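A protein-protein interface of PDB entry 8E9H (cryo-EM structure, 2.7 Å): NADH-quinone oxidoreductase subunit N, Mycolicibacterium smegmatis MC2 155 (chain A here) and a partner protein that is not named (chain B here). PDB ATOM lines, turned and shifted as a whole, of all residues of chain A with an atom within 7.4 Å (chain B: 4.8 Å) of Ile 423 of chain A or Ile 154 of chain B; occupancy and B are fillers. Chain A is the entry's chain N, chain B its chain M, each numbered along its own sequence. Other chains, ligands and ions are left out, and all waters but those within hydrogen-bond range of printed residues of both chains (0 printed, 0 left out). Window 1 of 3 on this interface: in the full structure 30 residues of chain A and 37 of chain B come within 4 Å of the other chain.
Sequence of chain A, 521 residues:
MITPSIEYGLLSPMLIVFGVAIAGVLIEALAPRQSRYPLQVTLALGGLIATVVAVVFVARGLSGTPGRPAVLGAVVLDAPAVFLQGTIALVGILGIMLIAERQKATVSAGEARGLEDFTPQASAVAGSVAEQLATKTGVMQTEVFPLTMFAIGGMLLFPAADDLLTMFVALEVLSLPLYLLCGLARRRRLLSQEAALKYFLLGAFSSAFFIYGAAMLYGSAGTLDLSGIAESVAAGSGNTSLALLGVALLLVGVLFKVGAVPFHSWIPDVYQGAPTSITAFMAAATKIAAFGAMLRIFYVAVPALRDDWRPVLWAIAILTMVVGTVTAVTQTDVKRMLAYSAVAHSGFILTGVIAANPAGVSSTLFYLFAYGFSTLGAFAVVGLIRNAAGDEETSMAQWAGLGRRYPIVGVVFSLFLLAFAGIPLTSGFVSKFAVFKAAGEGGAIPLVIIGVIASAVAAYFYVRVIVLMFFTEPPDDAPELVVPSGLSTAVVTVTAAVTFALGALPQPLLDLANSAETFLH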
ATOM      1  N   SER A 414      17.826  -6.080  31.252  1.00  0.00           N
ATOM      2  CA  SER A 414      17.935  -7.469  30.831  1.00  0.00           C
ATOM      3  C   SER A 414      16.572  -8.030  30.463  1.00  0.00           C
ATOM      4  O   SER A 414      16.448  -8.808  29.512  1.00  0.00           O
ATOM      5  CB  SER A 414      18.577  -8.302  31.937  1.00  0.00           C
ATOM      6  OG  SER A 414      17.621  -8.654  32.917  1.00  0.00           O
ATOM      7  N   LEU A 415      15.536  -7.655  31.210  1.00  0.00           N
ATOM      8  CA  LEU A 415      14.187  -8.086  30.869  1.00  0.00           C
ATOM      9  C   LEU A 415      13.796  -7.587  29.487  1.00  0.00           C
ATOM     10  O   LEU A 415      13.250  -8.338  28.673  1.00  0.00           O
ATOM     11  CB  LEU A 415      13.201  -7.584  31.923  1.00  0.00           C
ATOM     12  CG  LEU A 415      11.726  -7.572  31.523  1.00  0.00           C
ATOM     13  CD1 LEU A 415      11.239  -8.979  31.252  1.00  0.00           C
ATOM     14  CD2 LEU A 415      10.894  -6.920  32.605  1.00  0.00           C
ATOM     15  N   LEU A 417      15.830  -6.783  27.059  1.00  0.00           N
ATOM     16  CA  LEU A 417      16.655  -7.468  26.072  1.00  0.00           C
ATOM     17  C   LEU A 417      16.129  -8.867  25.797  1.00  0.00           C
ATOM     18  O   LEU A 417      16.093  -9.308  24.644  1.00  0.00           O
ATOM     19  CB  LEU A 417      18.101  -7.531  26.555  1.00  0.00           C
ATOM     20  CG  LEU A 417      18.843  -6.197  26.573  1.00  0.00           C
ATOM     21  CD1 LEU A 417      20.121  -6.331  27.368  1.00  0.00           C
ATOM     22  CD2 LEU A 417      19.138  -5.726  25.165  1.00  0.00           C
ATOM     23  N   LEU A 418      15.725  -9.585  26.842  1.00  0.00           N
ATOM     24  CA  LEU A 418      15.184 -10.922  26.640  1.00  0.00           C
ATOM     25  C   LEU A 418      13.838 -10.870  25.937  1.00  0.00           C
ATOM     26  O   LEU A 418      13.522 -11.760  25.140  1.00  0.00           O
ATOM     27  CB  LEU A 418      15.061 -11.651  27.974  1.00  0.00           C
ATOM     28  CG  LEU A 418      16.374 -11.858  28.731  1.00  0.00           C
ATOM     29  CD1 LEU A 418      16.101 -12.497  30.077  1.00  0.00           C
ATOM     30  CD2 LEU A 418      17.356 -12.688  27.927  1.00  0.00           C
ATOM     31  N   ALA A 419      13.036  -9.840  26.204  1.00  0.00           N
ATOM     32  CA  ALA A 419      11.802  -9.667  25.450  1.00  0.00           C
ATOM     33  C   ALA A 419      12.103  -9.498  23.970  1.00  0.00           C
ATOM     34  O   ALA A 419      11.476 -10.134  23.118  1.00  0.00           O
ATOM     35  CB  ALA A 419      11.026  -8.467  25.985  1.00  0.00           C
ATOM     36  N   PHE A 420      13.089  -8.665  23.644  1.00  0.00           N
ATOM     37  CA  PHE A 420      13.479  -8.529  22.246  1.00  0.00           C
ATOM     38  C   PHE A 420      13.964  -9.854  21.677  1.00  0.00           C
ATOM     39  O   PHE A 420      13.616 -10.206  20.547  1.00  0.00           O
ATOM     40  CB  PHE A 420      14.564  -7.469  22.089  1.00  0.00           C
ATOM     41  CG  PHE A 420      14.159  -6.112  22.573  1.00  0.00           C
ATOM     42  CD1 PHE A 420      12.888  -5.627  22.336  1.00  0.00           C
ATOM     43  CD2 PHE A 420      15.056  -5.315  23.255  1.00  0.00           C
ATOM     44  CE1 PHE A 420      12.520  -4.379  22.777  1.00  0.00           C
ATOM     45  CE2 PHE A 420      14.692  -4.066  23.698  1.00  0.00           C
ATOM     46  CZ  PHE A 420      13.423  -3.598  23.459  1.00  0.00           C
ATOM     47  N   ALA A 421      14.764 -10.599  22.440  1.00  0.00           N
ATOM     48  CA  ALA A 421      15.227 -11.899  21.971  1.00  0.00           C
ATOM     49  C   ALA A 421      14.078 -12.883  21.835  1.00  0.00           C
ATOM     50  O   ALA A 421      14.202 -13.889  21.130  1.00  0.00           O
ATOM     51  CB  ALA A 421      16.284 -12.452  22.923  1.00  0.00           C
ATOM     52  N   GLY A 422      12.958 -12.617  22.499  1.00  0.00           N
ATOM     53  CA  GLY A 422      11.818 -13.505  22.413  1.00  0.00           C
ATOM     54  C   GLY A 422      11.887 -14.691  23.344  1.00  0.00           C
ATOM     55  O   GLY A 422      11.406 -15.775  22.997  1.00  0.00           O
ATOM     56  N   ILE A 423      12.484 -14.524  24.516  1.00  0.00           N
ATOM     57  CA  ILE A 423      12.542 -15.628  25.480  1.00  0.00           C
ATOM     58  C   ILE A 423      11.161 -15.832  26.088  1.00  0.00           C
ATOM     59  O   ILE A 423      10.444 -14.845  26.328  1.00  0.00           O
ATOM     60  CB  ILE A 423      13.577 -15.334  26.563  1.00  0.00           C
ATOM     61  CG1 ILE A 423      14.938 -15.020  25.937  1.00  0.00           C
ATOM     62  CG2 ILE A 423      13.690 -16.510  27.509  1.00  0.00           C
ATOM     63  CD1 ILE A 423      15.411 -16.036  24.929  1.00  0.00           C
ATOM     64  N   PRO A 424      10.740 -17.069  26.355  1.00  0.00           N
ATOM     65  CA  PRO A 424       9.430 -17.279  26.984  1.00  0.00           C
ATOM     66  C   PRO A 424       9.296 -16.593  28.331  1.00  0.00           C
ATOM     67  O   PRO A 424      10.296 -16.223  28.952  1.00  0.00           O
ATOM     68  CB  PRO A 424       9.354 -18.803  27.114  1.00  0.00           C
ATOM     69  CG  PRO A 424      10.199 -19.300  26.008  1.00  0.00           C
ATOM     70  CD  PRO A 424      11.341 -18.341  25.924  1.00  0.00           C
ATOM     71  N   LEU A 425       8.052 -16.404  28.773  1.00  0.00           N
ATOM     72  CA  LEU A 425       7.722 -15.686  30.000  1.00  0.00           C
ATOM     73  C   LEU A 425       7.916 -14.185  29.833  1.00  0.00           C
ATOM     74  O   LEU A 425       7.674 -13.417  30.768  1.00  0.00           O
ATOM     75  CB  LEU A 425       8.548 -16.192  31.184  1.00  0.00           C
ATOM     76  CG  LEU A 425       8.448 -17.690  31.466  1.00  0.00           C
ATOM     77  CD1 LEU A 425       9.297 -18.056  32.668  1.00  0.00           C
ATOM     78  CD2 LEU A 425       7.002 -18.089  31.692  1.00  0.00           C
ATOM     79  N   THR A 426       8.348 -13.758  28.654  1.00  0.00           N
ATOM     80  CA  THR A 426       8.400 -12.347  28.314  1.00  0.00           C
ATOM     81  C   THR A 426       7.401 -12.061  27.207  1.00  0.00           C
ATOM     82  O   THR A 426       7.137 -12.909  26.351  1.00  0.00           O
ATOM     83  CB  THR A 426       9.798 -11.941  27.858  1.00  0.00           C
ATOM     84  OG1 THR A 426      10.041 -12.469  26.550  1.00  0.00           O
ATOM     85  CG2 THR A 426      10.849 -12.463  28.816  1.00  0.00           C
ATOM     86  N   SER A 427       6.845 -10.851  27.226  1.00  0.00           N
ATOM     87  CA  SER A 427       5.870 -10.492  26.205  1.00  0.00           C
ATOM     88  C   SER A 427       6.445 -10.690  24.815  1.00  0.00           C
ATOM     89  O   SER A 427       5.704 -10.978  23.871  1.00  0.00           O
ATOM     90  CB  SER A 427       5.424  -9.045  26.387  1.00  0.00           C
ATOM     91  OG  SER A 427       6.529  -8.167  26.307  1.00  0.00           O
ATOM     92  N   GLY A 428       7.762 -10.552  24.672  1.00  0.00           N
ATOM     93  CA  GLY A 428       8.396 -10.761  23.387  1.00  0.00           C
ATOM     94  C   GLY A 428       8.201 -12.150  22.822  1.00  0.00           C
ATOM     95  O   GLY A 428       7.997 -12.287  21.613  1.00  0.00           O
ATOM     96  N   PHE A 429       8.260 -13.186  23.658  1.00  0.00           N
ATOM     97  CA  PHE A 429       8.046 -14.534  23.146  1.00  0.00           C
ATOM     98  C   PHE A 429       6.608 -14.737  22.709  1.00  0.00           C
ATOM     99  O   PHE A 429       6.348 -15.310  21.650  1.00  0.00           O
ATOM    100  CB  PHE A 429       8.395 -15.588  24.183  1.00  0.00           C
ATOM    101  CG  PHE A 429       7.841 -16.935  23.838  1.00  0.00           C
ATOM    102  CD1 PHE A 429       8.351 -17.650  22.773  1.00  0.00           C
ATOM    103  CD2 PHE A 429       6.777 -17.463  24.542  1.00  0.00           C
ATOM    104  CE1 PHE A 429       7.833 -18.879  22.439  1.00  0.00           C
ATOM    105  CE2 PHE A 429       6.255 -18.691  24.212  1.00  0.00           C
ATOM    106  CZ  PHE A 429       6.784 -19.400  23.160  1.00  0.00           C
ATOM    107  N   VAL A 430       5.652 -14.330  23.543  1.00  0.00           N
ATOM    108  CA  VAL A 430       4.252 -14.449  23.152  1.00  0.00           C
ATOM    109  C   VAL A 430       4.042 -13.731  21.834  1.00  0.00           C
ATOM    110  O   VAL A 430       3.322 -14.200  20.947  1.00  0.00           O
ATOM    111  CB  VAL A 430       3.339 -13.881  24.253  1.00  0.00           C
ATOM    112  CG1 VAL A 430       1.887 -13.982  23.838  1.00  0.00           C
ATOM    113  CG2 VAL A 430       3.576 -14.605  25.563  1.00  0.00           C
ATOM    114  N   LYS A 432       6.333 -12.934  19.352  1.00  0.00           N
ATOM    115  CA  LYS A 432       6.933 -13.663  18.239  1.00  0.00           C
ATOM    116  C   LYS A 432       6.133 -14.910  17.907  1.00  0.00           C
ATOM    117  O   LYS A 432       5.959 -15.249  16.732  1.00  0.00           O
ATOM    118  CB  LYS A 432       8.374 -14.044  18.566  1.00  0.00           C
ATOM    119  CG  LYS A 432       9.389 -12.988  18.209  1.00  0.00           C
ATOM    120  CD  LYS A 432      10.800 -13.500  18.405  1.00  0.00           C
ATOM    121  CE  LYS A 432      11.817 -12.431  18.066  1.00  0.00           C
ATOM    122  NZ  LYS A 432      13.207 -12.852  18.379  1.00  0.00           N
ATOM    123  N   SER A 455      16.219 -15.196  14.899  1.00  0.00           N
ATOM    124  CA  SER A 455      16.105 -14.972  16.330  1.00  0.00           C
ATOM    125  C   SER A 455      17.237 -15.650  17.081  1.00  0.00           C
ATOM    126  O   SER A 455      17.760 -15.089  18.049  1.00  0.00           O
ATOM    127  CB  SER A 455      14.755 -15.483  16.826  1.00  0.00           C
ATOM    128  OG  SER A 455      14.521 -15.081  18.162  1.00  0.00           O
ATOM    129  N   ALA A 459      19.771 -13.475  19.375  1.00  0.00           N
ATOM    130  CA  ALA A 459      19.951 -13.759  20.789  1.00  0.00           C
ATOM    131  C   ALA A 459      21.386 -13.498  21.212  1.00  0.00           C
ATOM    132  O   ALA A 459      21.637 -13.085  22.345  1.00  0.00           O
ATOM    133  CB  ALA A 459      19.560 -15.205  21.085  1.00  0.00           C
ATOM    134  N   VAL A 463      22.321 -11.028  24.193  1.00  0.00           N
ATOM    135  CA  VAL A 463      22.881 -11.644  25.389  1.00  0.00           C
ATOM    136  C   VAL A 463      24.229 -11.032  25.730  1.00  0.00           C
ATOM    137  O   VAL A 463      24.627 -10.992  26.899  1.00  0.00           O
ATOM    138  CB  VAL A 463      22.984 -13.165  25.182  1.00  0.00           C
ATOM    139  CG1 VAL A 463      23.979 -13.768  26.141  1.00  0.00           C
ATOM    140  CG2 VAL A 463      21.622 -13.804  25.344  1.00  0.00           C
ATOM    141  N   ILE A 466      23.874  -8.381  28.288  1.00  0.00           N
ATOM    142  CA  ILE A 466      23.742  -8.894  29.646  1.00  0.00           C
ATOM    143  C   ILE A 466      25.090  -9.373  30.160  1.00  0.00           C
ATOM    144  O   ILE A 466      25.414  -9.211  31.342  1.00  0.00           O
ATOM    145  CB  ILE A 466      22.690 -10.015  29.691  1.00  0.00           C
ATOM    146  CG1 ILE A 466      21.333  -9.488  29.223  1.00  0.00           C
ATOM    147  CG2 ILE A 466      22.581 -10.576  31.094  1.00  0.00           C
ATOM    148  CD1 ILE A 466      20.311 -10.573  28.984  1.00  0.00           C
ATOM    149  N   PHE A 471      28.169 -10.014  34.071  1.00  0.00           N
ATOM    150  CA  PHE A 471      29.263 -10.958  34.230  1.00  0.00           C
ATOM    151  C   PHE A 471      30.634 -10.300  34.192  1.00  0.00           C
ATOM    152  O   PHE A 471      31.630 -10.964  34.498  1.00  0.00           O
ATOM    153  CB  PHE A 471      29.199 -12.025  33.134  1.00  0.00           C
ATOM    154  CG  PHE A 471      27.837 -12.635  32.954  1.00  0.00           C
ATOM    155  CD1 PHE A 471      26.889 -12.580  33.960  1.00  0.00           C
ATOM    156  CD2 PHE A 471      27.506 -13.257  31.769  1.00  0.00           C
ATOM    157  CE1 PHE A 471      25.646 -13.137  33.785  1.00  0.00           C
ATOM    158  CE2 PHE A 471      26.263 -13.811  31.590  1.00  0.00           C
ATOM    159  CZ  PHE A 471      25.331 -13.753  32.600  1.00  0.00           C
ATOM    160  N   GLY A 503       3.986 -11.184  29.091  1.00  0.00           N
ATOM    161  CA  GLY A 503       4.663 -12.444  28.887  1.00  0.00           C
ATOM    162  C   GLY A 503       4.048 -13.526  29.743  1.00  0.00           C
ATOM    163  O   GLY A 503       3.732 -14.616  29.258  1.00  0.00           O
ATOM    164  N   GLU B 150      12.405 -23.508  27.515  1.00  0.00           N
ATOM    165  CA  GLU B 150      13.257 -22.426  27.047  1.00  0.00           C
ATOM    166  C   GLU B 150      13.476 -21.360  28.109  1.00  0.00           C
ATOM    167  O   GLU B 150      14.540 -20.736  28.137  1.00  0.00           O
ATOM    168  CB  GLU B 150      12.658 -21.788  25.793  1.00  0.00           C
ATOM    169  N   ALA B 151      12.496 -21.136  28.987  1.00  0.00           N
ATOM    170  CA  ALA B 151      12.643 -20.111  30.012  1.00  0.00           C
ATOM    171  C   ALA B 151      13.728 -20.481  31.010  1.00  0.00           C
ATOM    172  O   ALA B 151      14.543 -19.637  31.391  1.00  0.00           O
ATOM    173  CB  ALA B 151      11.314 -19.898  30.730  1.00  0.00           C
ATOM    174  N   MET B 152      13.766 -21.745  31.435  1.00  0.00           N
ATOM    175  CA  MET B 152      14.732 -22.159  32.447  1.00  0.00           C
ATOM    176  C   MET B 152      16.175 -21.986  31.994  1.00  0.00           C
ATOM    177  O   MET B 152      17.089 -22.235  32.786  1.00  0.00           O
ATOM    178  CB  MET B 152      14.478 -23.613  32.845  1.00  0.00           C
ATOM    179  CG  MET B 152      15.036 -24.639  31.882  1.00  0.00           C
ATOM    180  SD  MET B 152      14.713 -26.319  32.435  1.00  0.00           S
ATOM    181  CE  MET B 152      15.218 -27.243  30.990  1.00  0.00           C
ATOM    182  N   LEU B 153      16.410 -21.577  30.748  1.00  0.00           N
ATOM    183  CA  LEU B 153      17.776 -21.309  30.322  1.00  0.00           C
ATOM    184  C   LEU B 153      18.311 -20.038  30.966  1.00  0.00           C
ATOM    185  O   LEU B 153      19.429 -20.027  31.492  1.00  0.00           O
ATOM    186  CB  LEU B 153      17.845 -21.193  28.800  1.00  0.00           C
ATOM    187  CG  LEU B 153      17.376 -22.391  27.978  1.00  0.00           C
ATOM    188  CD1 LEU B 153      17.493 -22.059  26.507  1.00  0.00           C
ATOM    189  CD2 LEU B 153      18.146 -23.643  28.321  1.00  0.00           C
ATOM    190  N   ILE B 154      17.526 -18.966  30.952  1.00  0.00           N
ATOM    191  CA  ILE B 154      18.035 -17.651  31.333  1.00  0.00           C
ATOM    192  C   ILE B 154      18.473 -17.634  32.794  1.00  0.00           C
ATOM    193  O   ILE B 154      19.537 -17.073  33.093  1.00  0.00           O
ATOM    194  CB  ILE B 154      17.017 -16.540  31.023  1.00  0.00           C
ATOM    195  CG1 ILE B 154      15.764 -16.625  31.897  1.00  0.00           C
ATOM    196  CG2 ILE B 154      16.628 -16.609  29.563  1.00  0.00           C
ATOM    197  CD1 ILE B 154      14.829 -15.451  31.745  1.00  0.00           C
ATOM    198  N   PRO B 155      17.724 -18.204  33.746  1.00  0.00           N
ATOM    199  CA  PRO B 155      18.227 -18.172  35.122  1.00  0.00           C
ATOM    200  C   PRO B 155      19.541 -18.907  35.248  1.00  0.00           C
ATOM    201  O   PRO B 155      20.448 -18.452  35.951  1.00  0.00           O
ATOM    202  CB  PRO B 155      17.106 -18.851  35.924  1.00  0.00           C
ATOM    203  CG  PRO B 155      15.950 -18.948  34.983  1.00  0.00           C
ATOM    204  CD  PRO B 155      16.586 -19.127  33.659  1.00  0.00           C
ATOM    205  N   MET B 156      19.679 -20.028  34.540  1.00  0.00           N
ATOM    206  CA  MET B 156      20.934 -20.764  34.559  1.00  0.00           C
ATOM    207  C   MET B 156      22.018 -20.006  33.813  1.00  0.00           C
ATOM    208  O   MET B 156      23.196 -20.074  34.173  1.00  0.00           O
ATOM    209  CB  MET B 156      20.731 -22.149  33.957  1.00  0.00           C
ATOM    210  CG  MET B 156      21.947 -23.034  34.048  1.00  0.00           C
ATOM    211  SD  MET B 156      22.221 -23.573  35.738  1.00  0.00           S
ATOM    212  CE  MET B 156      21.401 -25.156  35.695  1.00  0.00           C
ATOM    213  N   TYR B 157      21.641 -19.282  32.762  1.00  0.00           N
ATOM    214  CA  TYR B 157      22.601 -18.432  32.074  1.00  0.00           C
ATOM    215  C   TYR B 157      23.192 -17.406  33.030  1.00  0.00           C
ATOM    216  O   TYR B 157      24.414 -17.223  33.090  1.00  0.00           O
ATOM    217  CB  TYR B 157      21.912 -17.757  30.890  1.00  0.00           C
ATOM    218  CG  TYR B 157      22.549 -16.477  30.434  1.00  0.00           C
ATOM    219  CD1 TYR B 157      23.713 -16.481  29.685  1.00  0.00           C
ATOM    220  CD2 TYR B 157      21.975 -15.259  30.748  1.00  0.00           C
ATOM    221  CE1 TYR B 157      24.285 -15.303  29.266  1.00  0.00           C
ATOM    222  CE2 TYR B 157      22.539 -14.084  30.336  1.00  0.00           C
ATOM    223  CZ  TYR B 157      23.689 -14.108  29.595  1.00  0.00           C
ATOM    224  OH  TYR B 157      24.247 -12.921  29.195  1.00  0.00           O
ATOM    225  N   PHE B 158      22.336 -16.741  33.806  1.00  0.00           N
ATOM    226  CA  PHE B 158      22.824 -15.806  34.813  1.00  0.00           C
ATOM    227  C   PHE B 158      23.662 -16.523  35.858  1.00  0.00           C
ATOM    228  O   PHE B 158      24.727 -16.040  36.254  1.00  0.00           O
ATOM    229  CB  PHE B 158      21.651 -15.094  35.479  1.00  0.00           C
ATOM    230  CG  PHE B 158      21.136 -13.927  34.703  1.00  0.00           C
ATOM    231  CD1 PHE B 158      21.779 -12.707  34.755  1.00  0.00           C
ATOM    232  CD2 PHE B 158      20.005 -14.048  33.922  1.00  0.00           C
ATOM    233  CE1 PHE B 158      21.304 -11.632  34.043  1.00  0.00           C
ATOM    234  CE2 PHE B 158      19.527 -12.977  33.208  1.00  0.00           C
ATOM    235  CZ  PHE B 158      20.177 -11.768  33.268  1.00  0.00           C
ATOM    236  N   LEU B 176      24.028 -20.624  26.683  1.00  0.00           N
ATOM    237  CA  LEU B 176      22.738 -20.046  26.353  1.00  0.00           C
ATOM    238  C   LEU B 176      22.493 -20.109  24.859  1.00  0.00           C
ATOM    239  O   LEU B 176      21.383 -20.404  24.425  1.00  0.00           O
ATOM    240  CB  LEU B 176      22.650 -18.607  26.860  1.00  0.00           C
ATOM    241  CG  LEU B 176      21.329 -17.907  26.541  1.00  0.00           C
ATOM    242  CD1 LEU B 176      20.163 -18.689  27.111  1.00  0.00           C
ATOM    243  CD2 LEU B 176      21.335 -16.506  27.097  1.00  0.00           C
ATOM    244  N   LEU B 180      19.569 -22.185  23.243  1.00  0.00           N
ATOM    245  CA  LEU B 180      18.528 -21.330  22.701  1.00  0.00           C
ATOM    246  C   LEU B 180      18.370 -21.520  21.203  1.00  0.00           C
ATOM    247  O   LEU B 180      17.258 -21.404  20.688  1.00  0.00           O
ATOM    248  CB  LEU B 180      18.848 -19.874  23.026  1.00  0.00           C
ATOM    249  CG  LEU B 180      17.728 -18.863  22.827  1.00  0.00           C
ATOM    250  CD1 LEU B 180      16.514 -19.240  23.654  1.00  0.00           C
ATOM    251  CD2 LEU B 180      18.223 -17.485  23.202  1.00  0.00           C
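OH of Tyr 157 of chain B is in hydrogen-bond range of O of Val 463 of chain A.
O of Ile 423 of chain A is in hydrogen-bond range of OG1 of Thr 426 of chain A (2.4 Å).
N of Ile 423 of chain A is in hydrogen-bond range of O of Leu 418 of chain A (3.0 Å).
Leu 418 of chain A touches Ile 154 of chain B (CD1 to CD1, 3.6 Å).
Ile 154 of chain B touches Ile 423 of chain A.
CD1 of Ile 423 of chain A touches CD2 of Leu 180 of chain B (3.6 Å).
CG of Pro 424 of chain A touches CB of Glu 150 of chain B, at 3.5 Å.
Ala 151 of chain B touches Leu 425 of chain A (CB to CD1, 3.3 Å).
CD2 of Leu 180 of chain B touches CB of Ala 459 of chain A (3.4 Å).
Leu 176 of chain B touches Val 463 of chain A (CD2 to CG2, 3.2 Å).
CB of Ile 466 of chain A touches OH of Tyr 157 of chain B, at 3.3 Å.
CG2 of Ile 466 of chain A touches CE1 of Phe 158 of chain B (3.4 Å).
CE1 of Phe 471 of chain A touches O of Phe 158 of chain B, 3.9 Å away.
Leu 417 of chain A touches none of the printed residues of chain B.
Of chain B, only Ile 154 and Leu 180 come within 4 Å of Ile 423 of chain A.
Of the printed residues of chain B, Pro 424 of chain A touches Glu 150 (3.5 Å).
Lys 432 of chain A touches none of the printed residues of chain B.
Printed residues of chain B within 4 Å of Val 463 of chain A: Tyr 157 (3.0 Å) and Leu 176 (3.2 Å).
Printed residues of chain A within 4 Å of Glu 150 of chain B: Pro 424.
Ile 154 of chain B touches just these residues of chain A: Leu 418 and Ile 423.
Printed residues of chain A within 4 Å of Tyr 157 of chain B: Val 463 (3.0 Å), Ile 466 (3.3 Å) and Phe 471 (3.3 Å).
Of the printed residues of chain A, Leu 176 of chain B touches Val 463 (3.2 Å).
The nearest residue of chain B that does not touch Ile 423 of chain A is Glu 150 of chain B (4.4 Å).
The nearest residue of chain A that does not touch Ile 154 of chain B is Pro 424 of chain A (5.4 Å).
The nearest printed residue of chain B that does not touch Val 463 of chain A is Leu 180 of chain B (5.4 Å).
Of the 23 printed residues of chain A, 8 touch a printed residue of chain B.
Hydrophobic or aromatic side chains of chain A that line the printed part of chain B: Leu 418, Ile 423, Pro 424, Leu 425, Ala 459, Val 463, Ile 466 and Phe 471.
Of the 11 printed residues of chain B, 7 touch a printed residue of chain A.
Printed residues of chain B that touch a printed residue of chain A: Glu 150, Ala 151, Ile 154, Tyr 157, Phe 158, Leu 176 and Leu 180.
Among the printed residues, no Asp or Glu carboxylate lies within 4 Å of a Lys or Arg side-chain nitrogen of the other chain.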
